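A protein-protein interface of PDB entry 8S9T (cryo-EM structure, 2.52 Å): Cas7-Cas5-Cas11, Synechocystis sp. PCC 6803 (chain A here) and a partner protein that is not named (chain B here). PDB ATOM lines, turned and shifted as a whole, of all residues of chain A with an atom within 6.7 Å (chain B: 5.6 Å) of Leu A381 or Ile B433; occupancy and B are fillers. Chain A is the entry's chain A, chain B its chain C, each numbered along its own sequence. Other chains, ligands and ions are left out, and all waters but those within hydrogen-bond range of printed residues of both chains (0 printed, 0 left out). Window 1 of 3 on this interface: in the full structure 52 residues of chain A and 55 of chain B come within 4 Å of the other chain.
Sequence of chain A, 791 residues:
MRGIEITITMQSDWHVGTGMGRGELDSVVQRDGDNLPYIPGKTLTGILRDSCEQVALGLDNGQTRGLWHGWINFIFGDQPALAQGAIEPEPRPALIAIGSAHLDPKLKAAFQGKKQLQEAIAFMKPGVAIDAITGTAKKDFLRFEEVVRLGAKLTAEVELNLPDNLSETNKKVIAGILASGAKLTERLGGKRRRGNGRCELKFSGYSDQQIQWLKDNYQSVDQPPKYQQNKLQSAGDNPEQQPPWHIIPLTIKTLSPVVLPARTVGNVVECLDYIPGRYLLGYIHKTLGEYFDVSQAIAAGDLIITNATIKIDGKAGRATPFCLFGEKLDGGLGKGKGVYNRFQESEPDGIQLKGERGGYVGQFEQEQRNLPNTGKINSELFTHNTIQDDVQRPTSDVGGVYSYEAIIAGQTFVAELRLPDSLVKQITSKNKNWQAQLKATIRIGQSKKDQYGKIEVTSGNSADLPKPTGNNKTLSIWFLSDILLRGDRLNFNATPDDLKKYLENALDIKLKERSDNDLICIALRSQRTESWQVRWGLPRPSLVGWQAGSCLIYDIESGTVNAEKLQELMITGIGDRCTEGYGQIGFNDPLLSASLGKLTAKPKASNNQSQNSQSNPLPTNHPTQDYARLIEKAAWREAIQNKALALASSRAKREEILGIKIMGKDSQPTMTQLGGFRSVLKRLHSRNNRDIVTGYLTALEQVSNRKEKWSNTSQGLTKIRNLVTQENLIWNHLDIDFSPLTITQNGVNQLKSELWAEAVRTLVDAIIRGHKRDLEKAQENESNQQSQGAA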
ATOM      1  N   VAL A 268       8.767 -19.574  -7.268  1.00  0.00           N
ATOM      2  CA  VAL A 268       8.178 -19.816  -5.957  1.00  0.00           C
ATOM      3  C   VAL A 268       8.443 -21.251  -5.528  1.00  0.00           C
ATOM      4  O   VAL A 268       8.411 -22.171  -6.347  1.00  0.00           O
ATOM      5  CB  VAL A 268       6.665 -19.473  -5.933  1.00  0.00           C
ATOM      6  CG1 VAL A 268       5.920 -20.195  -7.008  1.00  0.00           C
ATOM      7  CG2 VAL A 268       6.056 -19.791  -4.583  1.00  0.00           C
ATOM      8  N   VAL A 269       8.745 -21.429  -4.246  1.00  0.00           N
ATOM      9  CA  VAL A 269       8.823 -22.737  -3.604  1.00  0.00           C
ATOM     10  C   VAL A 269       7.690 -22.845  -2.592  1.00  0.00           C
ATOM     11  O   VAL A 269       7.618 -22.057  -1.644  1.00  0.00           O
ATOM     12  CB  VAL A 269      10.191 -22.967  -2.943  1.00  0.00           C
ATOM     13  CG1 VAL A 269      10.249 -24.315  -2.303  1.00  0.00           C
ATOM     14  CG2 VAL A 269      11.279 -22.862  -3.970  1.00  0.00           C
ATOM     15  N   GLU A 270       6.809 -23.820  -2.796  1.00  0.00           N
ATOM     16  CA  GLU A 270       5.832 -24.218  -1.794  1.00  0.00           C
ATOM     17  C   GLU A 270       6.434 -25.159  -0.757  1.00  0.00           C
ATOM     18  O   GLU A 270       7.343 -25.937  -1.042  1.00  0.00           O
ATOM     19  CB  GLU A 270       4.632 -24.872  -2.467  1.00  0.00           C
ATOM     20  CG  GLU A 270       4.008 -23.982  -3.517  1.00  0.00           C
ATOM     21  CD  GLU A 270       2.730 -24.542  -4.086  1.00  0.00           C
ATOM     22  OE1 GLU A 270       1.933 -25.116  -3.316  1.00  0.00           O
ATOM     23  OE2 GLU A 270       2.523 -24.415  -5.309  1.00  0.00           O
ATOM     24  N   SER A 379       2.030 -21.597   7.981  1.00  0.00           N
ATOM     25  CA  SER A 379       3.000 -21.293   6.949  1.00  0.00           C
ATOM     26  C   SER A 379       2.837 -19.849   6.512  1.00  0.00           C
ATOM     27  O   SER A 379       1.738 -19.296   6.549  1.00  0.00           O
ATOM     28  CB  SER A 379       2.823 -22.220   5.753  1.00  0.00           C
ATOM     29  OG  SER A 379       3.822 -22.008   4.781  1.00  0.00           O
ATOM     30  N   GLU A 380       3.945 -19.221   6.148  1.00  0.00           N
ATOM     31  CA  GLU A 380       3.906 -17.881   5.595  1.00  0.00           C
ATOM     32  C   GLU A 380       4.706 -17.850   4.304  1.00  0.00           C
ATOM     33  O   GLU A 380       5.670 -18.594   4.140  1.00  0.00           O
ATOM     34  CB  GLU A 380       4.435 -16.858   6.588  1.00  0.00           C
ATOM     35  CG  GLU A 380       4.157 -15.443   6.186  1.00  0.00           C
ATOM     36  CD  GLU A 380       2.666 -15.226   5.914  1.00  0.00           C
ATOM     37  OE1 GLU A 380       1.922 -14.973   6.885  1.00  0.00           O
ATOM     38  OE2 GLU A 380       2.245 -15.265   4.736  1.00  0.00           O
ATOM     39  N   LEU A 381       4.300 -16.987   3.385  1.00  0.00           N
ATOM     40  CA  LEU A 381       5.059 -16.730   2.170  1.00  0.00           C
ATOM     41  C   LEU A 381       6.102 -15.643   2.404  1.00  0.00           C
ATOM     42  O   LEU A 381       5.782 -14.556   2.884  1.00  0.00           O
ATOM     43  CB  LEU A 381       4.132 -16.354   1.021  1.00  0.00           C
ATOM     44  CG  LEU A 381       4.835 -16.316  -0.328  1.00  0.00           C
ATOM     45  CD1 LEU A 381       5.013 -17.696  -0.878  1.00  0.00           C
ATOM     46  CD2 LEU A 381       4.048 -15.456  -1.277  1.00  0.00           C
ATOM     47  N   PHE A 382       7.355 -15.963   2.117  1.00  0.00           N
ATOM     48  CA  PHE A 382       8.455 -15.016   2.184  1.00  0.00           C
ATOM     49  C   PHE A 382       8.900 -14.662   0.776  1.00  0.00           C
ATOM     50  O   PHE A 382       9.016 -15.536  -0.077  1.00  0.00           O
ATOM     51  CB  PHE A 382       9.601 -15.596   2.996  1.00  0.00           C
ATOM     52  CG  PHE A 382       9.240 -15.837   4.416  1.00  0.00           C
ATOM     53  CD1 PHE A 382       8.621 -17.006   4.782  1.00  0.00           C
ATOM     54  CD2 PHE A 382       9.477 -14.888   5.380  1.00  0.00           C
ATOM     55  CE1 PHE A 382       8.268 -17.224   6.065  1.00  0.00           C
ATOM     56  CE2 PHE A 382       9.131 -15.116   6.672  1.00  0.00           C
ATOM     57  CZ  PHE A 382       8.523 -16.283   7.013  1.00  0.00           C
ATOM     58  N   THR A 383       9.157 -13.390   0.537  1.00  0.00           N
ATOM     59  CA  THR A 383       9.516 -12.917  -0.787  1.00  0.00           C
ATOM     60  C   THR A 383      10.872 -12.231  -0.761  1.00  0.00           C
ATOM     61  O   THR A 383      11.193 -11.494   0.169  1.00  0.00           O
ATOM     62  CB  THR A 383       8.420 -11.973  -1.312  1.00  0.00           C
ATOM     63  OG1 THR A 383       7.175 -12.677  -1.376  1.00  0.00           O
ATOM     64  CG2 THR A 383       8.726 -11.483  -2.666  1.00  0.00           C
ATOM     65  N   SER A 403       9.860 -16.309  -4.153  1.00  0.00           N
ATOM     66  CA  SER A 403       9.140 -16.522  -2.904  1.00  0.00           C
ATOM     67  C   SER A 403       9.317 -17.933  -2.377  1.00  0.00           C
ATOM     68  O   SER A 403       9.399 -18.883  -3.150  1.00  0.00           O
ATOM     69  CB  SER A 403       7.639 -16.258  -3.046  1.00  0.00           C
ATOM     70  OG  SER A 403       7.354 -14.968  -3.532  1.00  0.00           O
ATOM     71  N   TYR A 404       9.397 -18.046  -1.053  1.00  0.00           N
ATOM     72  CA  TYR A 404       9.368 -19.309  -0.321  1.00  0.00           C
ATOM     73  C   TYR A 404       8.197 -19.328   0.647  1.00  0.00           C
ATOM     74  O   TYR A 404       8.043 -18.403   1.440  1.00  0.00           O
ATOM     75  CB  TYR A 404      10.654 -19.530   0.477  1.00  0.00           C
ATOM     76  CG  TYR A 404      11.912 -19.671  -0.323  1.00  0.00           C
ATOM     77  CD1 TYR A 404      11.882 -20.161  -1.607  1.00  0.00           C
ATOM     78  CD2 TYR A 404      13.135 -19.364   0.225  1.00  0.00           C
ATOM     79  CE1 TYR A 404      13.010 -20.292  -2.339  1.00  0.00           C
ATOM     80  CE2 TYR A 404      14.280 -19.515  -0.494  1.00  0.00           C
ATOM     81  CZ  TYR A 404      14.215 -19.984  -1.782  1.00  0.00           C
ATOM     82  OH  TYR A 404      15.361 -20.157  -2.512  1.00  0.00           O
ATOM     83  N   GLU A 405       7.373 -20.372   0.592  1.00  0.00           N
ATOM     84  CA  GLU A 405       6.616 -20.751   1.780  1.00  0.00           C
ATOM     85  C   GLU A 405       7.545 -21.353   2.823  1.00  0.00           C
ATOM     86  O   GLU A 405       8.423 -22.153   2.506  1.00  0.00           O
ATOM     87  CB  GLU A 405       5.507 -21.745   1.461  1.00  0.00           C
ATOM     88  CG  GLU A 405       4.437 -21.224   0.576  1.00  0.00           C
ATOM     89  CD  GLU A 405       3.269 -22.175   0.476  1.00  0.00           C
ATOM     90  OE1 GLU A 405       3.415 -23.349   0.854  1.00  0.00           O
ATOM     91  OE2 GLU A 405       2.186 -21.735   0.034  1.00  0.00           O
ATOM     92  N   ALA A 406       7.327 -20.991   4.077  1.00  0.00           N
ATOM     93  CA  ALA A 406       8.036 -21.617   5.170  1.00  0.00           C
ATOM     94  C   ALA A 406       7.082 -21.881   6.318  1.00  0.00           C
ATOM     95  O   ALA A 406       6.157 -21.112   6.559  1.00  0.00           O
ATOM     96  CB  ALA A 406       9.194 -20.747   5.637  1.00  0.00           C
ATOM     97  N   TYR A 452      16.590 -19.220   7.187  1.00  0.00           N
ATOM     98  CA  TYR A 452      15.721 -20.381   7.170  1.00  0.00           C
ATOM     99  C   TYR A 452      16.384 -21.574   7.842  1.00  0.00           C
ATOM    100  O   TYR A 452      17.603 -21.727   7.812  1.00  0.00           O
ATOM    101  CB  TYR A 452      15.339 -20.747   5.758  1.00  0.00           C
ATOM    102  CG  TYR A 452      14.573 -19.680   5.064  1.00  0.00           C
ATOM    103  CD1 TYR A 452      13.305 -19.328   5.479  1.00  0.00           C
ATOM    104  CD2 TYR A 452      15.132 -18.993   4.005  1.00  0.00           C
ATOM    105  CE1 TYR A 452      12.610 -18.338   4.842  1.00  0.00           C
ATOM    106  CE2 TYR A 452      14.451 -18.016   3.366  1.00  0.00           C
ATOM    107  CZ  TYR A 452      13.189 -17.690   3.780  1.00  0.00           C
ATOM    108  OH  TYR A 452      12.511 -16.702   3.130  1.00  0.00           O
ATOM    109  N   PHE B 383       2.924 -13.949  -6.898  1.00  0.00           N
ATOM    110  CA  PHE B 383       2.328 -14.893  -5.971  1.00  0.00           C
ATOM    111  C   PHE B 383       1.902 -16.162  -6.713  1.00  0.00           C
ATOM    112  O   PHE B 383       1.441 -16.087  -7.853  1.00  0.00           O
ATOM    113  CB  PHE B 383       1.132 -14.220  -5.285  1.00  0.00           C
ATOM    114  CG  PHE B 383       0.493 -15.035  -4.211  1.00  0.00           C
ATOM    115  CD1 PHE B 383      -0.435 -16.004  -4.528  1.00  0.00           C
ATOM    116  CD2 PHE B 383       0.816 -14.839  -2.890  1.00  0.00           C
ATOM    117  CE1 PHE B 383      -1.010 -16.758  -3.566  1.00  0.00           C
ATOM    118  CE2 PHE B 383       0.238 -15.598  -1.924  1.00  0.00           C
ATOM    119  CZ  PHE B 383      -0.677 -16.562  -2.267  1.00  0.00           C
ATOM    120  N   PRO B 384       2.067 -17.338  -6.107  1.00  0.00           N
ATOM    121  CA  PRO B 384       1.633 -18.597  -6.747  1.00  0.00           C
ATOM    122  C   PRO B 384       0.135 -18.674  -7.025  1.00  0.00           C
ATOM    123  O   PRO B 384      -0.680 -18.675  -6.110  1.00  0.00           O
ATOM    124  CB  PRO B 384       2.076 -19.662  -5.740  1.00  0.00           C
ATOM    125  CG  PRO B 384       2.271 -18.936  -4.463  1.00  0.00           C
ATOM    126  CD  PRO B 384       2.717 -17.577  -4.808  1.00  0.00           C
ATOM    127  N   VAL B 387      -1.766 -21.356  -5.180  1.00  0.00           N
ATOM    128  CA  VAL B 387      -2.171 -21.037  -3.822  1.00  0.00           C
ATOM    129  C   VAL B 387      -3.313 -20.039  -3.822  1.00  0.00           C
ATOM    130  O   VAL B 387      -4.243 -20.141  -3.018  1.00  0.00           O
ATOM    131  CB  VAL B 387      -0.945 -20.518  -3.044  1.00  0.00           C
ATOM    132  CG1 VAL B 387      -1.305 -20.084  -1.652  1.00  0.00           C
ATOM    133  CG2 VAL B 387       0.121 -21.578  -2.987  1.00  0.00           C
ATOM    134  N   LEU B 391      -7.207 -20.465  -2.236  1.00  0.00           N
ATOM    135  CA  LEU B 391      -7.876 -19.508  -1.373  1.00  0.00           C
ATOM    136  C   LEU B 391      -9.215 -19.051  -1.943  1.00  0.00           C
ATOM    137  O   LEU B 391     -10.185 -18.900  -1.197  1.00  0.00           O
ATOM    138  CB  LEU B 391      -6.948 -18.327  -1.129  1.00  0.00           C
ATOM    139  CG  LEU B 391      -7.462 -17.206  -0.254  1.00  0.00           C
ATOM    140  CD1 LEU B 391      -7.857 -17.742   1.093  1.00  0.00           C
ATOM    141  CD2 LEU B 391      -6.386 -16.178  -0.122  1.00  0.00           C
ATOM    142  N   LEU B 427      -3.760 -10.446  -0.480  1.00  0.00           N
ATOM    143  CA  LEU B 427      -2.673 -11.179   0.159  1.00  0.00           C
ATOM    144  C   LEU B 427      -1.482 -10.266   0.429  1.00  0.00           C
ATOM    145  O   LEU B 427      -0.458 -10.287  -0.244  1.00  0.00           O
ATOM    146  CB  LEU B 427      -2.284 -12.410  -0.646  1.00  0.00           C
ATOM    147  CG  LEU B 427      -3.365 -13.466  -0.436  1.00  0.00           C
ATOM    148  CD1 LEU B 427      -4.604 -13.301  -1.329  1.00  0.00           C
ATOM    149  CD2 LEU B 427      -2.823 -14.849  -0.440  1.00  0.00           C
ATOM    150  N   ASP B 429       1.609  -8.995   2.949  1.00  0.00           N
ATOM    151  CA  ASP B 429       2.820  -9.785   3.136  1.00  0.00           C
ATOM    152  C   ASP B 429       2.727 -10.768   4.299  1.00  0.00           C
ATOM    153  O   ASP B 429       3.135 -11.928   4.168  1.00  0.00           O
ATOM    154  CB  ASP B 429       4.012  -8.853   3.335  1.00  0.00           C
ATOM    155  CG  ASP B 429       5.320  -9.602   3.427  1.00  0.00           C
ATOM    156  OD1 ASP B 429       5.858  -9.977   2.367  1.00  0.00           O
ATOM    157  OD2 ASP B 429       5.816  -9.814   4.549  1.00  0.00           O
ATOM    158  N   SER B 431      -0.129 -11.725   5.930  1.00  0.00           N
ATOM    159  CA  SER B 431      -1.555 -11.909   6.135  1.00  0.00           C
ATOM    160  C   SER B 431      -1.955 -13.375   6.226  1.00  0.00           C
ATOM    161  O   SER B 431      -3.123 -13.667   6.479  1.00  0.00           O
ATOM    162  CB  SER B 431      -2.330 -11.223   5.006  1.00  0.00           C
ATOM    163  OG  SER B 431      -3.713 -11.161   5.293  1.00  0.00           O
ATOM    164  N   GLY B 432      -1.016 -14.292   6.077  1.00  0.00           N
ATOM    165  CA  GLY B 432      -1.328 -15.671   5.790  1.00  0.00           C
ATOM    166  C   GLY B 432      -1.625 -15.904   4.322  1.00  0.00           C
ATOM    167  O   GLY B 432      -1.850 -14.987   3.542  1.00  0.00           O
ATOM    168  N   ILE B 433      -1.596 -17.173   3.941  1.00  0.00           N
ATOM    169  CA  ILE B 433      -1.762 -17.563   2.547  1.00  0.00           C
ATOM    170  C   ILE B 433      -2.787 -18.677   2.422  1.00  0.00           C
ATOM    171  O   ILE B 433      -3.212 -19.020   1.318  1.00  0.00           O
ATOM    172  CB  ILE B 433      -0.409 -17.976   1.931  1.00  0.00           C
ATOM    173  CG1 ILE B 433       0.266 -19.057   2.775  1.00  0.00           C
ATOM    174  CG2 ILE B 433       0.487 -16.781   1.721  1.00  0.00           C
ATOM    175  CD1 ILE B 433       1.588 -19.466   2.266  1.00  0.00           C
ATOM    176  N   ASP B 434      -3.198 -19.241   3.547  1.00  0.00           N
ATOM    177  CA  ASP B 434      -4.294 -20.192   3.584  1.00  0.00           C
ATOM    178  C   ASP B 434      -5.438 -19.621   4.403  1.00  0.00           C
ATOM    179  O   ASP B 434      -5.224 -18.837   5.327  1.00  0.00           O
ATOM    180  CB  ASP B 434      -3.846 -21.545   4.138  1.00  0.00           C
ATOM    181  CG  ASP B 434      -3.504 -21.491   5.593  1.00  0.00           C
ATOM    182  OD1 ASP B 434      -4.427 -21.591   6.423  1.00  0.00           O
ATOM    183  OD2 ASP B 434      -2.303 -21.348   5.915  1.00  0.00           O
ATOM    184  N   PHE B 435      -6.656 -20.014   4.029  1.00  0.00           N
ATOM    185  CA  PHE B 435      -7.867 -19.364   4.518  1.00  0.00           C
ATOM    186  C   PHE B 435      -7.960 -19.363   6.037  1.00  0.00           C
ATOM    187  O   PHE B 435      -8.262 -18.333   6.647  1.00  0.00           O
ATOM    188  CB  PHE B 435      -9.087 -20.052   3.905  1.00  0.00           C
ATOM    189  CG  PHE B 435     -10.382 -19.465   4.334  1.00  0.00           C
ATOM    190  CD1 PHE B 435     -10.888 -18.343   3.707  1.00  0.00           C
ATOM    191  CD2 PHE B 435     -11.105 -20.033   5.357  1.00  0.00           C
ATOM    192  CE1 PHE B 435     -12.069 -17.796   4.112  1.00  0.00           C
ATOM    193  CE2 PHE B 435     -12.281 -19.484   5.759  1.00  0.00           C
ATOM    194  CZ  PHE B 435     -12.765 -18.366   5.137  1.00  0.00           C
ATOM    195  N   ARG B 437      -5.591 -19.709   8.301  1.00  0.00           N
ATOM    196  CA  ARG B 437      -4.555 -18.864   8.878  1.00  0.00           C
ATOM    197  C   ARG B 437      -4.844 -17.388   8.652  1.00  0.00           C
ATOM    198  O   ARG B 437      -4.628 -16.566   9.546  1.00  0.00           O
ATOM    199  CB  ARG B 437      -3.210 -19.245   8.279  1.00  0.00           C
ATOM    200  CG  ARG B 437      -2.044 -18.542   8.866  1.00  0.00           C
ATOM    201  CD  ARG B 437      -2.035 -18.691  10.340  1.00  0.00           C
ATOM    202  NE  ARG B 437      -0.838 -18.113  10.908  1.00  0.00           N
ATOM    203  CZ  ARG B 437      -0.678 -17.877  12.198  1.00  0.00           C
ATOM    204  NH1 ARG B 437       0.418 -17.280  12.631  1.00  0.00           N
ATOM    205  NH2 ARG B 437      -1.636 -18.197  13.043  1.00  0.00           N
ATOM    206  N   ILE B 438      -5.332 -17.035   7.466  1.00  0.00           N
ATOM    207  CA  ILE B 438      -5.721 -15.656   7.194  1.00  0.00           C
ATOM    208  C   ILE B 438      -6.735 -15.162   8.216  1.00  0.00           C
ATOM    209  O   ILE B 438      -6.559 -14.107   8.829  1.00  0.00           O
ATOM    210  CB  ILE B 438      -6.266 -15.528   5.762  1.00  0.00           C
ATOM    211  CG1 ILE B 438      -5.132 -15.618   4.750  1.00  0.00           C
ATOM    212  CG2 ILE B 438      -7.040 -14.239   5.618  1.00  0.00           C
ATOM    213  CD1 ILE B 438      -5.565 -16.025   3.402  1.00  0.00           C
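N of Glu A405 lies within hydrogen-bond range of O of Val A269 (2.8 Å). The backbone NH (N) of Ala A406 is in hydrogen-bond range of the backbone carbonyl oxygen (O) of Glu A380 (2.9 Å).
The side-chain carboxylate of Glu A380 lies within hydrogen-bond range of the backbone NH of Gly B432, at 3.1 Å.
Among the printed residues, pairs that only touch across the chains: Val A268 with Pro B384 (3.9 Å), Glu A270 with Val B387 (3.99 Å), Glu A380 with Asp B429 (3.5 Å), Glu A380 with Ser B431 (3.96 Å), Glu A380 with Ile B433 (3.8 Å), Leu A381 with Phe B383 (3.7 Å), Leu A381 with Asp B429 (3.9 Å), Leu A381 with Ile B433 (3.7 Å), Glu A405 with Val B387 (3.7 Å) and Glu A405 with Ile B433 (3.2 Å).
Of the 13 printed residues of chain A, 5 touch a printed residue of chain B. Hydrophobic or aromatic side chains of chain A within 4 Å of the printed part of chain B: Val A268 and Leu A381. Of the 13 printed residues of chain B, 7 touch a printed residue of chain A. Printed residues of chain B that touch a printed residue of chain A: Phe B383, Pro B384, Val B387, Asp B429, Ser B431, Gly B432 and Ile B433. Among the printed residues, 11 pairs touch across the chains. Among the printed residues, no Asp or Glu carboxylate lies within 4 Å of a Lys or Arg side-chain nitrogen of the other chain.
Of the printed residues of chain B, Leu A381 touches Phe B383, Asp B429 and Ile B433. Of chain A, only Glu A380, Leu A381 and Glu A405 come within 4 Å of Ile B433. Of the printed residues of chain B, Glu A380 touches Asp B429 (3.5 Å), Ser B431 (3.96 Å), Gly B432 (3.1 Å) and Ile B433 (3.8 Å). Of the printed residues of chain A, Pro B384 touches Val A268. Phe B435 touches none of the printed residues of chain A. Tyr A404 touches none of the printed residues of chain B.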
